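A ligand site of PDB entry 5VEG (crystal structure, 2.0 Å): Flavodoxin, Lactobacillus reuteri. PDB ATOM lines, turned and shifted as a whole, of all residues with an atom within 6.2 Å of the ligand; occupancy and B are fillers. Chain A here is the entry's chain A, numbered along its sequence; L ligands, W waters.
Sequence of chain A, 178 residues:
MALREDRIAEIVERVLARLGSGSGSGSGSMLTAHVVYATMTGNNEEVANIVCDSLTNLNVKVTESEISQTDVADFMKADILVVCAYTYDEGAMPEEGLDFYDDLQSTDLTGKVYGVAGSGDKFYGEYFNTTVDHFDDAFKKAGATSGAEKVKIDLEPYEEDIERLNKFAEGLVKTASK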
ATOM      1  N   ALA A  38      21.944  -4.219  -7.823  1.00  0.00           N
ATOM      2  CA  ALA A  38      21.768  -4.232  -9.262  1.00  0.00           C
ATOM      3  C   ALA A  38      21.688  -5.686  -9.694  1.00  0.00           C
ATOM      4  O   ALA A  38      22.454  -6.524  -9.206  1.00  0.00           O
ATOM      5  CB  ALA A  38      22.903  -3.524  -9.986  1.00  0.00           C
ATOM      6  N   THR A  39      20.743  -5.996 -10.587  1.00  0.00           N
ATOM      7  CA  THR A  39      20.570  -7.397 -10.906  1.00  0.00           C
ATOM      8  C   THR A  39      19.873  -7.546 -12.245  1.00  0.00           C
ATOM      9  O   THR A  39      19.130  -6.661 -12.691  1.00  0.00           O
ATOM     10  CB  THR A  39      19.791  -8.121  -9.795  1.00  0.00           C
ATOM     11  OG1 THR A  39      19.791  -9.529 -10.054  1.00  0.00           O
ATOM     12  CG2 THR A  39      18.357  -7.609  -9.696  1.00  0.00           C
ATOM     13  N   MET A  40      20.122  -8.696 -12.883  1.00  0.00           N
ATOM     14  CA  MET A  40      19.392  -9.073 -14.099  1.00  0.00           C
ATOM     15  C   MET A  40      18.710 -10.420 -13.981  1.00  0.00           C
ATOM     16  O   MET A  40      17.569 -10.564 -14.422  1.00  0.00           O
ATOM     17  CB  MET A  40      20.338  -9.052 -15.298  1.00  0.00           C
ATOM     18  CG  MET A  40      20.785  -7.648 -15.619  1.00  0.00           C
ATOM     19  SD  MET A  40      21.398  -7.448 -17.293  1.00  0.00           S
ATOM     20  CE  MET A  40      22.400  -8.889 -17.382  1.00  0.00           C
ATOM     21  N   THR A  41      19.356 -11.407 -13.361  1.00  0.00           N
ATOM     22  CA  THR A  41      18.748 -12.719 -13.188  1.00  0.00           C
ATOM     23  C   THR A  41      18.499 -13.039 -11.719  1.00  0.00           C
ATOM     24  O   THR A  41      18.225 -14.205 -11.388  1.00  0.00           O
ATOM     25  CB  THR A  41      19.590 -13.798 -13.862  1.00  0.00           C
ATOM     26  OG1 THR A  41      20.988 -13.534 -13.663  1.00  0.00           O
ATOM     27  CG2 THR A  41      19.313 -13.822 -15.364  1.00  0.00           C
ATOM     28  N   GLY A  42      18.577 -12.040 -10.838  1.00  0.00           N
ATOM     29  CA  GLY A  42      18.129 -12.161  -9.473  1.00  0.00           C
ATOM     30  C   GLY A  42      19.162 -12.552  -8.453  1.00  0.00           C
ATOM     31  O   GLY A  42      18.875 -12.491  -7.252  1.00  0.00           O
ATOM     32  N   ASN A  43      20.366 -12.976  -8.873  1.00  0.00           N
ATOM     33  CA  ASN A  43      21.340 -13.467  -7.902  1.00  0.00           C
ATOM     34  C   ASN A  43      21.757 -12.370  -6.926  1.00  0.00           C
ATOM     35  O   ASN A  43      21.854 -12.608  -5.723  1.00  0.00           O
ATOM     36  CB  ASN A  43      22.579 -14.032  -8.623  1.00  0.00           C
ATOM     37  CG  ASN A  43      22.292 -15.393  -9.282  1.00  0.00           C
ATOM     38  OD1 ASN A  43      21.344 -16.076  -8.915  1.00  0.00           O
ATOM     39  ND2 ASN A  43      23.113 -15.754 -10.269  1.00  0.00           N
ATOM     40  N   ASN A  44      22.020 -11.164  -7.424  1.00  0.00           N
ATOM     41  CA  ASN A  44      22.454 -10.079  -6.558  1.00  0.00           C
ATOM     42  C   ASN A  44      21.317  -9.486  -5.752  1.00  0.00           C
ATOM     43  O   ASN A  44      21.570  -8.894  -4.689  1.00  0.00           O
ATOM     44  CB  ASN A  44      23.129  -8.998  -7.381  1.00  0.00           C
ATOM     45  CG  ASN A  44      24.544  -9.366  -7.722  1.00  0.00           C
ATOM     46  OD1 ASN A  44      25.453  -9.112  -6.935  1.00  0.00           O
ATOM     47  ND2 ASN A  44      24.745 -10.007  -8.875  1.00  0.00           N
ATOM     48  N   GLU A  45      20.073  -9.620  -6.218  1.00  0.00           N
ATOM     49  CA  GLU A  45      18.933  -9.295  -5.370  1.00  0.00           C
ATOM     50  C   GLU A  45      18.788 -10.323  -4.252  1.00  0.00           C
ATOM     51  O   GLU A  45      18.465  -9.971  -3.117  1.00  0.00           O
ATOM     52  CB  GLU A  45      17.658  -9.210  -6.209  1.00  0.00           C
ATOM     53  CG  GLU A  45      16.423  -9.023  -5.358  1.00  0.00           C
ATOM     54  CD  GLU A  45      15.159  -8.856  -6.174  1.00  0.00           C
ATOM     55  OE1 GLU A  45      15.250  -8.738  -7.418  1.00  0.00           O
ATOM     56  OE2 GLU A  45      14.083  -8.806  -5.539  1.00  0.00           O
ATOM     57  N   TYR A  86      26.217  -6.912  -9.754  1.00  0.00           N
ATOM     58  CA  TYR A  86      26.876  -7.888 -10.612  1.00  0.00           C
ATOM     59  C   TYR A  86      27.993  -7.234 -11.418  1.00  0.00           C
ATOM     60  O   TYR A  86      28.151  -6.010 -11.446  1.00  0.00           O
ATOM     61  CB  TYR A  86      25.862  -8.538 -11.569  1.00  0.00           C
ATOM     62  CG  TYR A  86      25.226  -7.544 -12.542  1.00  0.00           C
ATOM     63  CD1 TYR A  86      25.857  -7.188 -13.732  1.00  0.00           C
ATOM     64  CD2 TYR A  86      23.987  -6.963 -12.254  1.00  0.00           C
ATOM     65  CE1 TYR A  86      25.268  -6.267 -14.624  1.00  0.00           C
ATOM     66  CE2 TYR A  86      23.399  -6.039 -13.122  1.00  0.00           C
ATOM     67  CZ  TYR A  86      24.038  -5.704 -14.304  1.00  0.00           C
ATOM     68  OH  TYR A  86      23.454  -4.793 -15.162  1.00  0.00           O
ATOM     69  N   THR A  87      28.761  -8.088 -12.102  1.00  0.00           N
ATOM     70  CA  THR A  87      29.755  -7.706 -13.087  1.00  0.00           C
ATOM     71  C   THR A  87      29.374  -8.352 -14.413  1.00  0.00           C
ATOM     72  O   THR A  87      28.907  -9.501 -14.450  1.00  0.00           O
ATOM     73  CB  THR A  87      31.156  -8.170 -12.647  1.00  0.00           C
ATOM     74  OG1 THR A  87      31.473  -7.608 -11.356  1.00  0.00           O
ATOM     75  CG2 THR A  87      32.199  -7.727 -13.658  1.00  0.00           C
ATOM     76  N   TYR A  88      29.571  -7.625 -15.512  1.00  0.00           N
ATOM     77  CA  TYR A  88      29.152  -8.078 -16.835  1.00  0.00           C
ATOM     78  C   TYR A  88      30.285  -7.912 -17.832  1.00  0.00           C
ATOM     79  O   TYR A  88      31.312  -7.292 -17.536  1.00  0.00           O
ATOM     80  CB  TYR A  88      27.909  -7.318 -17.320  1.00  0.00           C
ATOM     81  CG  TYR A  88      26.883  -8.203 -17.996  1.00  0.00           C
ATOM     82  CD1 TYR A  88      26.364  -9.305 -17.345  1.00  0.00           C
ATOM     83  CD2 TYR A  88      26.427  -7.913 -19.276  1.00  0.00           C
ATOM     84  CE1 TYR A  88      25.413 -10.110 -17.956  1.00  0.00           C
ATOM     85  CE2 TYR A  88      25.478  -8.699 -19.902  1.00  0.00           C
ATOM     86  CZ  TYR A  88      24.977  -9.800 -19.227  1.00  0.00           C
ATOM     87  OH  TYR A  88      24.028 -10.591 -19.840  1.00  0.00           O
ATOM     88  N   ASP A  89      30.108  -8.506 -19.013  1.00  0.00           N
ATOM     89  CA  ASP A  89      30.952  -8.286 -20.188  1.00  0.00           C
ATOM     90  C   ASP A  89      32.418  -8.036 -19.839  1.00  0.00           C
ATOM     91  O   ASP A  89      33.000  -7.007 -20.173  1.00  0.00           O
ATOM     92  CB  ASP A  89      30.415  -7.117 -21.021  1.00  0.00           C
ATOM     93  CG  ASP A  89      29.250  -7.504 -21.874  1.00  0.00           C
ATOM     94  OD1 ASP A  89      29.443  -8.279 -22.827  1.00  0.00           O
ATOM     95  OD2 ASP A  89      28.144  -7.010 -21.603  1.00  0.00           O
ATOM     96  N   GLU A  90      32.990  -8.998 -19.130  1.00  0.00           N
ATOM     97  CA  GLU A  90      34.419  -8.973 -18.815  1.00  0.00           C
ATOM     98  C   GLU A  90      34.789  -7.723 -18.011  1.00  0.00           C
ATOM     99  O   GLU A  90      35.579  -6.877 -18.447  1.00  0.00           O
ATOM    100  CB  GLU A  90      35.252  -9.094 -20.097  1.00  0.00           C
ATOM    101  CG  GLU A  90      34.913 -10.334 -20.948  1.00  0.00           C
ATOM    102  CD  GLU A  90      33.650 -10.166 -21.801  1.00  0.00           C
ATOM    103  OE1 GLU A  90      33.664  -9.362 -22.761  1.00  0.00           O
ATOM    104  OE2 GLU A  90      32.640 -10.838 -21.502  1.00  0.00           O
ATOM    105  N   GLY A  91      34.221  -7.624 -16.820  1.00  0.00           N
ATOM    106  CA  GLY A  91      34.597  -6.576 -15.872  1.00  0.00           C
ATOM    107  C   GLY A  91      33.737  -5.331 -15.886  1.00  0.00           C
ATOM    108  O   GLY A  91      34.036  -4.385 -15.149  1.00  0.00           O
ATOM    109  N   ALA A  92      32.675  -5.306 -16.690  1.00  0.00           N
ATOM    110  CA  ALA A  92      31.882  -4.093 -16.849  1.00  0.00           C
ATOM    111  C   ALA A  92      30.994  -3.864 -15.620  1.00  0.00           C
ATOM    112  O   ALA A  92      30.456  -4.809 -15.040  1.00  0.00           O
ATOM    113  CB  ALA A  92      31.017  -4.184 -18.108  1.00  0.00           C
ATOM    114  N   SER A 119      27.456 -11.128  -6.500  1.00  0.00           N
ATOM    115  CA  SER A 119      27.467 -12.439  -7.129  1.00  0.00           C
ATOM    116  C   SER A 119      27.991 -12.270  -8.540  1.00  0.00           C
ATOM    117  O   SER A 119      27.562 -11.366  -9.262  1.00  0.00           O
ATOM    118  CB  SER A 119      26.069 -13.064  -7.147  1.00  0.00           C
ATOM    119  OG  SER A 119      26.000 -14.091  -8.143  1.00  0.00           O
ATOM    120  N   GLY A 120      28.964 -13.103  -8.917  1.00  0.00           N
ATOM    121  CA  GLY A 120      29.517 -13.060 -10.229  1.00  0.00           C
ATOM    122  C   GLY A 120      29.872 -14.483 -10.631  1.00  0.00           C
ATOM    123  O   GLY A 120      29.326 -15.446 -10.081  1.00  0.00           O
ATOM    124  N   ASP A 121      30.826 -14.632 -11.530  1.00  0.00           N
ATOM    125  CA  ASP A 121      31.157 -15.941 -12.094  1.00  0.00           C
ATOM    126  C   ASP A 121      32.664 -16.086 -12.095  1.00  0.00           C
ATOM    127  O   ASP A 121      33.353 -15.361 -12.833  1.00  0.00           O
ATOM    128  CB  ASP A 121      30.567 -16.079 -13.499  1.00  0.00           C
ATOM    129  CG  ASP A 121      30.691 -17.495 -14.055  1.00  0.00           C
ATOM    130  OD1 ASP A 121      31.647 -18.193 -13.663  1.00  0.00           O
ATOM    131  OD2 ASP A 121      29.827 -17.900 -14.888  1.00  0.00           O
ATOM    132  N   LYS A 122      33.180 -17.035 -11.310  1.00  0.00           N
ATOM    133  CA  LYS A 122      34.629 -17.253 -11.228  1.00  0.00           C
ATOM    134  C   LYS A 122      35.254 -17.624 -12.579  1.00  0.00           C
ATOM    135  O   LYS A 122      36.463 -17.450 -12.744  1.00  0.00           O
ATOM    136  CB  LYS A 122      34.957 -18.323 -10.189  1.00  0.00           C
ATOM    137  CG  LYS A 122      34.680 -17.839  -8.774  1.00  0.00           C
ATOM    138  CD  LYS A 122      35.121 -18.798  -7.664  1.00  0.00           C
ATOM    139  CE  LYS A 122      34.763 -18.222  -6.295  1.00  0.00           C
ATOM    140  NZ  LYS A 122      35.131 -19.124  -5.160  1.00  0.00           N
ATOM    141  N   TYR A 124      35.276 -15.971 -15.127  1.00  0.00           N
ATOM    142  CA  TYR A 124      35.872 -14.767 -15.704  1.00  0.00           C
ATOM    143  C   TYR A 124      37.169 -14.367 -15.021  1.00  0.00           C
ATOM    144  O   TYR A 124      37.695 -13.275 -15.281  1.00  0.00           O
ATOM    145  CB  TYR A 124      34.861 -13.604 -15.690  1.00  0.00           C
ATOM    146  CG  TYR A 124      33.679 -13.903 -16.585  1.00  0.00           C
ATOM    147  CD1 TYR A 124      33.695 -13.529 -17.927  1.00  0.00           C
ATOM    148  CD2 TYR A 124      32.595 -14.638 -16.118  1.00  0.00           C
ATOM    149  CE1 TYR A 124      32.634 -13.837 -18.773  1.00  0.00           C
ATOM    150  CE2 TYR A 124      31.529 -14.937 -16.961  1.00  0.00           C
ATOM    151  CZ  TYR A 124      31.565 -14.548 -18.281  1.00  0.00           C
ATOM    152  OH  TYR A 124      30.505 -14.846 -19.116  1.00  0.00           O
ATOM    153  N   TYR A 127      38.479 -10.965 -13.780  1.00  0.00           N
ATOM    154  CA  TYR A 127      37.310 -10.107 -13.868  1.00  0.00           C
ATOM    155  C   TYR A 127      36.197 -10.552 -12.930  1.00  0.00           C
ATOM    156  O   TYR A 127      35.080 -10.036 -13.022  1.00  0.00           O
ATOM    157  CB  TYR A 127      36.812 -10.048 -15.314  1.00  0.00           C
ATOM    158  CG  TYR A 127      37.781  -9.284 -16.194  1.00  0.00           C
ATOM    159  CD1 TYR A 127      38.156  -7.984 -15.878  1.00  0.00           C
ATOM    160  CD2 TYR A 127      38.350  -9.876 -17.306  1.00  0.00           C
ATOM    161  CE1 TYR A 127      39.052  -7.282 -16.664  1.00  0.00           C
ATOM    162  CE2 TYR A 127      39.250  -9.191 -18.106  1.00  0.00           C
ATOM    163  CZ  TYR A 127      39.589  -7.891 -17.777  1.00  0.00           C
ATOM    164  OH  TYR A 127      40.488  -7.211 -18.564  1.00  0.00           O
ATOM    165  N   PHE A 128      36.470 -11.526 -12.054  1.00  0.00           N
ATOM    166  CA  PHE A 128      35.504 -11.999 -11.072  1.00  0.00           C
ATOM    167  C   PHE A 128      35.037 -10.893 -10.139  1.00  0.00           C
ATOM    168  O   PHE A 128      35.818 -10.381  -9.339  1.00  0.00           O
ATOM    169  CB  PHE A 128      36.103 -13.142 -10.249  1.00  0.00           C
ATOM    170  CG  PHE A 128      35.150 -13.741  -9.230  1.00  0.00           C
ATOM    171  CD1 PHE A 128      33.898 -14.179  -9.622  1.00  0.00           C
ATOM    172  CD2 PHE A 128      35.538 -13.883  -7.898  1.00  0.00           C
ATOM    173  CE1 PHE A 128      33.009 -14.736  -8.690  1.00  0.00           C
ATOM    174  CE2 PHE A 128      34.683 -14.449  -6.952  1.00  0.00           C
ATOM    175  CZ  PHE A 128      33.416 -14.872  -7.347  1.00  0.00           C
ATOM    176  N   ASN A 129      33.765 -10.527 -10.222  1.00  0.00           N
ATOM    177  CA  ASN A 129      33.156  -9.566  -9.275  1.00  0.00           C
ATOM    178  C   ASN A 129      33.920  -8.245  -9.216  1.00  0.00           C
ATOM    179  O   ASN A 129      34.048  -7.637  -8.162  1.00  0.00           O
ATOM    180  CB  ASN A 129      33.047 -10.183  -7.864  1.00  0.00           C
ATOM    181  CG  ASN A 129      31.714 -10.874  -7.653  1.00  0.00           C
ATOM    182  OD1 ASN A 129      30.674 -10.322  -8.000  1.00  0.00           O
ATOM    183  ND2 ASN A 129      31.742 -12.076  -7.105  1.00  0.00           N
ATOM    184  N   THR A 130      34.437  -7.779 -10.356  1.00  0.00           N
ATOM    185  CA  THR A 130      35.171  -6.515 -10.358  1.00  0.00           C
ATOM    186  C   THR A 130      34.284  -5.349  -9.904  1.00  0.00           C
ATOM    187  O   THR A 130      34.787  -4.340  -9.402  1.00  0.00           O
ATOM    188  CB  THR A 130      35.732  -6.203 -11.743  1.00  0.00           C
ATOM    189  OG1 THR A 130      34.669  -6.196 -12.705  1.00  0.00           O
ATOM    190  CG2 THR A 130      36.730  -7.234 -12.162  1.00  0.00           C
ATOM    191  N   ILE A 153      30.758 -13.590  -4.307  1.00  0.00           N
ATOM    192  CA  ILE A 153      30.027 -14.838  -4.382  1.00  0.00           C
ATOM    193  C   ILE A 153      30.066 -15.356  -5.809  1.00  0.00           C
ATOM    194  O   ILE A 153      30.002 -14.571  -6.773  1.00  0.00           O
ATOM    195  CB  ILE A 153      28.588 -14.635  -3.878  1.00  0.00           C
ATOM    196  CG1 ILE A 153      28.608 -14.477  -2.349  1.00  0.00           C
ATOM    197  CG2 ILE A 153      27.684 -15.805  -4.290  1.00  0.00           C
ATOM    198  CD1 ILE A 153      27.470 -13.652  -1.804  1.00  0.00           C
ATOM    199  N   ASP A 154      30.183 -16.677  -5.959  1.00  0.00           N
ATOM    200  CA  ASP A 154      30.134 -17.322  -7.265  1.00  0.00           C
ATOM    201  C   ASP A 154      28.690 -17.752  -7.544  1.00  0.00           C
ATOM    202  O   ASP A 154      28.197 -18.706  -6.934  1.00  0.00           O
ATOM    203  CB  ASP A 154      31.097 -18.499  -7.317  1.00  0.00           C
ATOM    204  CG  ASP A 154      31.145 -19.162  -8.692  1.00  0.00           C
ATOM    205  OD1 ASP A 154      31.405 -18.479  -9.698  1.00  0.00           O
ATOM    206  OD2 ASP A 154      30.924 -20.387  -8.766  1.00  0.00           O
ATOM    207  N   LEU A 155      28.020 -17.039  -8.452  1.00  0.00           N
ATOM    208  CA  LEU A 155      26.688 -17.390  -8.952  1.00  0.00           C
ATOM    209  C   LEU A 155      25.705 -17.348  -7.792  1.00  0.00           C
ATOM    210  O   LEU A 155      25.616 -16.305  -7.101  1.00  0.00           O
ATOM    211  CB  LEU A 155      26.759 -18.736  -9.697  1.00  0.00           C
ATOM    212  CG  LEU A 155      27.603 -18.820 -10.964  1.00  0.00           C
ATOM    213  CD1 LEU A 155      27.343 -20.163 -11.668  1.00  0.00           C
ATOM    214  CD2 LEU A 155      27.328 -17.664 -11.923  1.00  0.00           C
ATOM    215  N   GLU A 156      24.933 -18.407  -7.541  1.00  0.00           N
ATOM    216  CA  GLU A 156      23.896 -18.344  -6.528  1.00  0.00           C
ATOM    217  C   GLU A 156      24.506 -18.487  -5.145  1.00  0.00           C
ATOM    218  O   GLU A 156      25.465 -19.256  -4.961  1.00  0.00           O
ATOM    219  CB  GLU A 156      22.861 -19.437  -6.753  1.00  0.00           C
ATOM    220  CG  GLU A 156      21.490 -18.873  -7.085  1.00  0.00           C
ATOM    221  CD  GLU A 156      20.408 -19.922  -7.129  1.00  0.00           C
ATOM    222  OE1 GLU A 156      19.941 -20.323  -6.029  1.00  0.00           O
ATOM    223  OE2 GLU A 156      20.018 -20.323  -8.242  1.00  0.00           O
HETATM  224  N1  LIG L   1      30.754 -12.244 -13.722  1.00  0.00           N
HETATM  225  C1  LIG L   1      31.952 -11.733 -13.245  1.00  0.00           C
HETATM  226  O1  LIG L   1      32.247 -11.887 -12.067  1.00  0.00           O
HETATM  227  N2  LIG L   1      32.810 -11.056 -14.089  1.00  0.00           N
HETATM  228  C2  LIG L   1      32.493 -10.896 -15.425  1.00  0.00           C
HETATM  229  O2  LIG L   1      33.276 -10.291 -16.149  1.00  0.00           O
HETATM  230  C3  LIG L   1      31.296 -11.410 -15.926  1.00  0.00           C
HETATM  231  N3  LIG L   1      30.949 -11.259 -17.252  1.00  0.00           N
HETATM  232  C4  LIG L   1      29.748 -11.793 -17.700  1.00  0.00           C
HETATM  233  C5  LIG L   1      29.371 -11.654 -19.040  1.00  0.00           C
HETATM  234  C6  LIG L   1      28.164 -12.189 -19.496  1.00  0.00           C
HETATM  235  C7  LIG L   1      27.751 -12.060 -20.934  1.00  0.00           C
HETATM  236  C8  LIG L   1      27.323 -12.869 -18.615  1.00  0.00           C
HETATM  237  C9  LIG L   1      26.023 -13.446 -19.101  1.00  0.00           C
HETATM  238  C10 LIG L   1      27.695 -13.009 -17.283  1.00  0.00           C
HETATM  239  C11 LIG L   1      28.892 -12.452 -16.835  1.00  0.00           C
HETATM  240  N4  LIG L   1      29.235 -12.595 -15.506  1.00  0.00           N
HETATM  241  C12 LIG L   1      30.431 -12.089 -15.053  1.00  0.00           C
HETATM  242  C13 LIG L   1      28.338 -13.378 -14.591  1.00  0.00           C
HETATM  243  C14 LIG L   1      27.300 -12.611 -13.781  1.00  0.00           C
HETATM  244  O3  LIG L   1      27.955 -11.626 -13.030  1.00  0.00           O
HETATM  245  C15 LIG L   1      26.731 -13.642 -12.827  1.00  0.00           C
HETATM  246  O4  LIG L   1      25.961 -14.616 -13.521  1.00  0.00           O
HETATM  247  C16 LIG L   1      25.872 -13.036 -11.742  1.00  0.00           C
HETATM  248  O5  LIG L   1      25.485 -14.061 -10.858  1.00  0.00           O
HETATM  249  C17 LIG L   1      24.617 -12.415 -12.333  1.00  0.00           C
HETATM  250  O6  LIG L   1      23.988 -11.716 -11.283  1.00  0.00           O
HETATM  251  P1  LIG L   1      22.433 -11.285 -11.388  1.00  0.00           P
HETATM  252  O7  LIG L   1      21.606 -12.555 -11.418  1.00  0.00           O
HETATM  253  O8  LIG L   1      22.118 -10.494 -10.125  1.00  0.00           O
HETATM  254  O9  LIG L   1      22.194 -10.522 -12.644  1.00  0.00           O
HETATM  255  O   HOH W   1      24.514 -14.252 -15.734  1.00  0.00           O
HETATM  256  O   HOH W   2      22.632 -12.538 -15.338  1.00  0.00           O
HETATM  257  O   HOH W   3      23.831  -9.894 -14.723  1.00  0.00           O
HETATM  258  O   HOH W   4      24.047 -17.093 -13.003  1.00  0.00           O
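N3 of the ligand lies close to N of Asp 89 (3.4 Å). An oxygen (O7) of the ligand sits at hydrogen-bond distance from the backbone NH of Gly 42 (3.1 Å). ND2 of Asn 43 lies within hydrogen-bond range of O5 of the ligand. The backbone NH (N) of Asp 121 lies within hydrogen-bond range of an oxygen (O1) of the ligand (3.1 Å). An oxygen (O9) of the ligand sits at hydrogen-bond distance from the backbone NH of Thr 41. N of Asn 129 sits at hydrogen-bond distance from O1 of the ligand. The side-chain hydroxyl of Thr 39 lies within hydrogen-bond range of an oxygen (O8) of the ligand (2.5 Å). A nitrogen (N2) of the ligand sits at hydrogen-bond distance from the backbone carbonyl oxygen of Tyr 127 (2.7 Å). An oxygen (O7) of the ligand lies within hydrogen-bond range of the backbone NH (N) of Asn 43. An oxygen (O9) of the ligand sits at hydrogen-bond distance from the backbone NH (N) of Met 40 (2.8 Å). The side-chain hydroxyl (OG) of Ser 119 lies within hydrogen-bond range of an oxygen (O5) of the ligand, 2.8 Å away. O3 of the ligand is in hydrogen-bond range of O of Thr 87 (2.7 Å). OG1 of Thr 41 sits at hydrogen-bond distance from O7 of the ligand, at 2.5 Å. N of Gly 91 is in hydrogen-bond range of O2 of the ligand (2.9 Å). N of Asn 44 sits at hydrogen-bond distance from O8 of the ligand, at 2.8 Å. An oxygen (O2) of the ligand sits close to the backbone NH (N) of Glu 90, 3.3 Å away. ND2 of Asn 44 lies within hydrogen-bond range of O8 of the ligand, at 2.9 Å.
The backbone carbonyl oxygen (O) of Ile 153 is in hydrogen-bond range of the side-chain amide nitrogen (ND2) of Asn 129. The backbone carbonyl oxygen of Gly 91 lies within hydrogen-bond range of the side-chain hydroxyl of Thr 130, at 3.1 Å. The backbone carbonyl oxygen (O) of Gly 120 sits at hydrogen-bond distance from the backbone NH (N) of Leu 155. The backbone NH (N) of Gly 120 lies within hydrogen-bond range of the backbone carbonyl oxygen (O) of Ile 153 (2.8 Å). N of Gly 120 is in hydrogen-bond range of OD1 of Asn 129, 3.4 Å away. OG1 of Thr 87 lies within hydrogen-bond range of N of Thr 130 (3.1 Å). The backbone NH (N) of Ser 119 sits at hydrogen-bond distance from the side-chain amide oxygen (OD1) of Asn 44 (2.9 Å). OG of Ser 119 lies within hydrogen-bond range of O of Leu 155.
Water W4 lies within hydrogen-bond range of O4 of the ligand (3.2 Å) and ND2 of Asn 43 (3.2 Å). Water W2 lies within hydrogen-bond range of the side-chain hydroxyl (OG1) of Thr 41 and an oxygen (O9) of the ligand.
Residues that only touch the ligand: Tyr 124, Phe 128, Tyr 88, Gly 120, Tyr 86 and Leu 155. Hydrophobic or aromatic side chains within 4 Å of the ligand: Met 40, Tyr 86, Tyr 88, Tyr 124, Tyr 127, Phe 128 and Leu 155. Within 4 Å of the ligand: Thr 39, Met 40, Thr 41, Gly 42, Asn 43, Asn 44, Tyr 86, Thr 87, Tyr 88, Asp 89, Glu 90, Gly 91, Ser 119, Gly 120, Asp 121, Tyr 124, Tyr 127, Phe 128, Asn 129 and Leu 155. Along chain A the residues within 4 Å of the ligand span positions 39 to 155. The nearest printed residue that does not touch the ligand is Ala 38 (4.1 Å).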
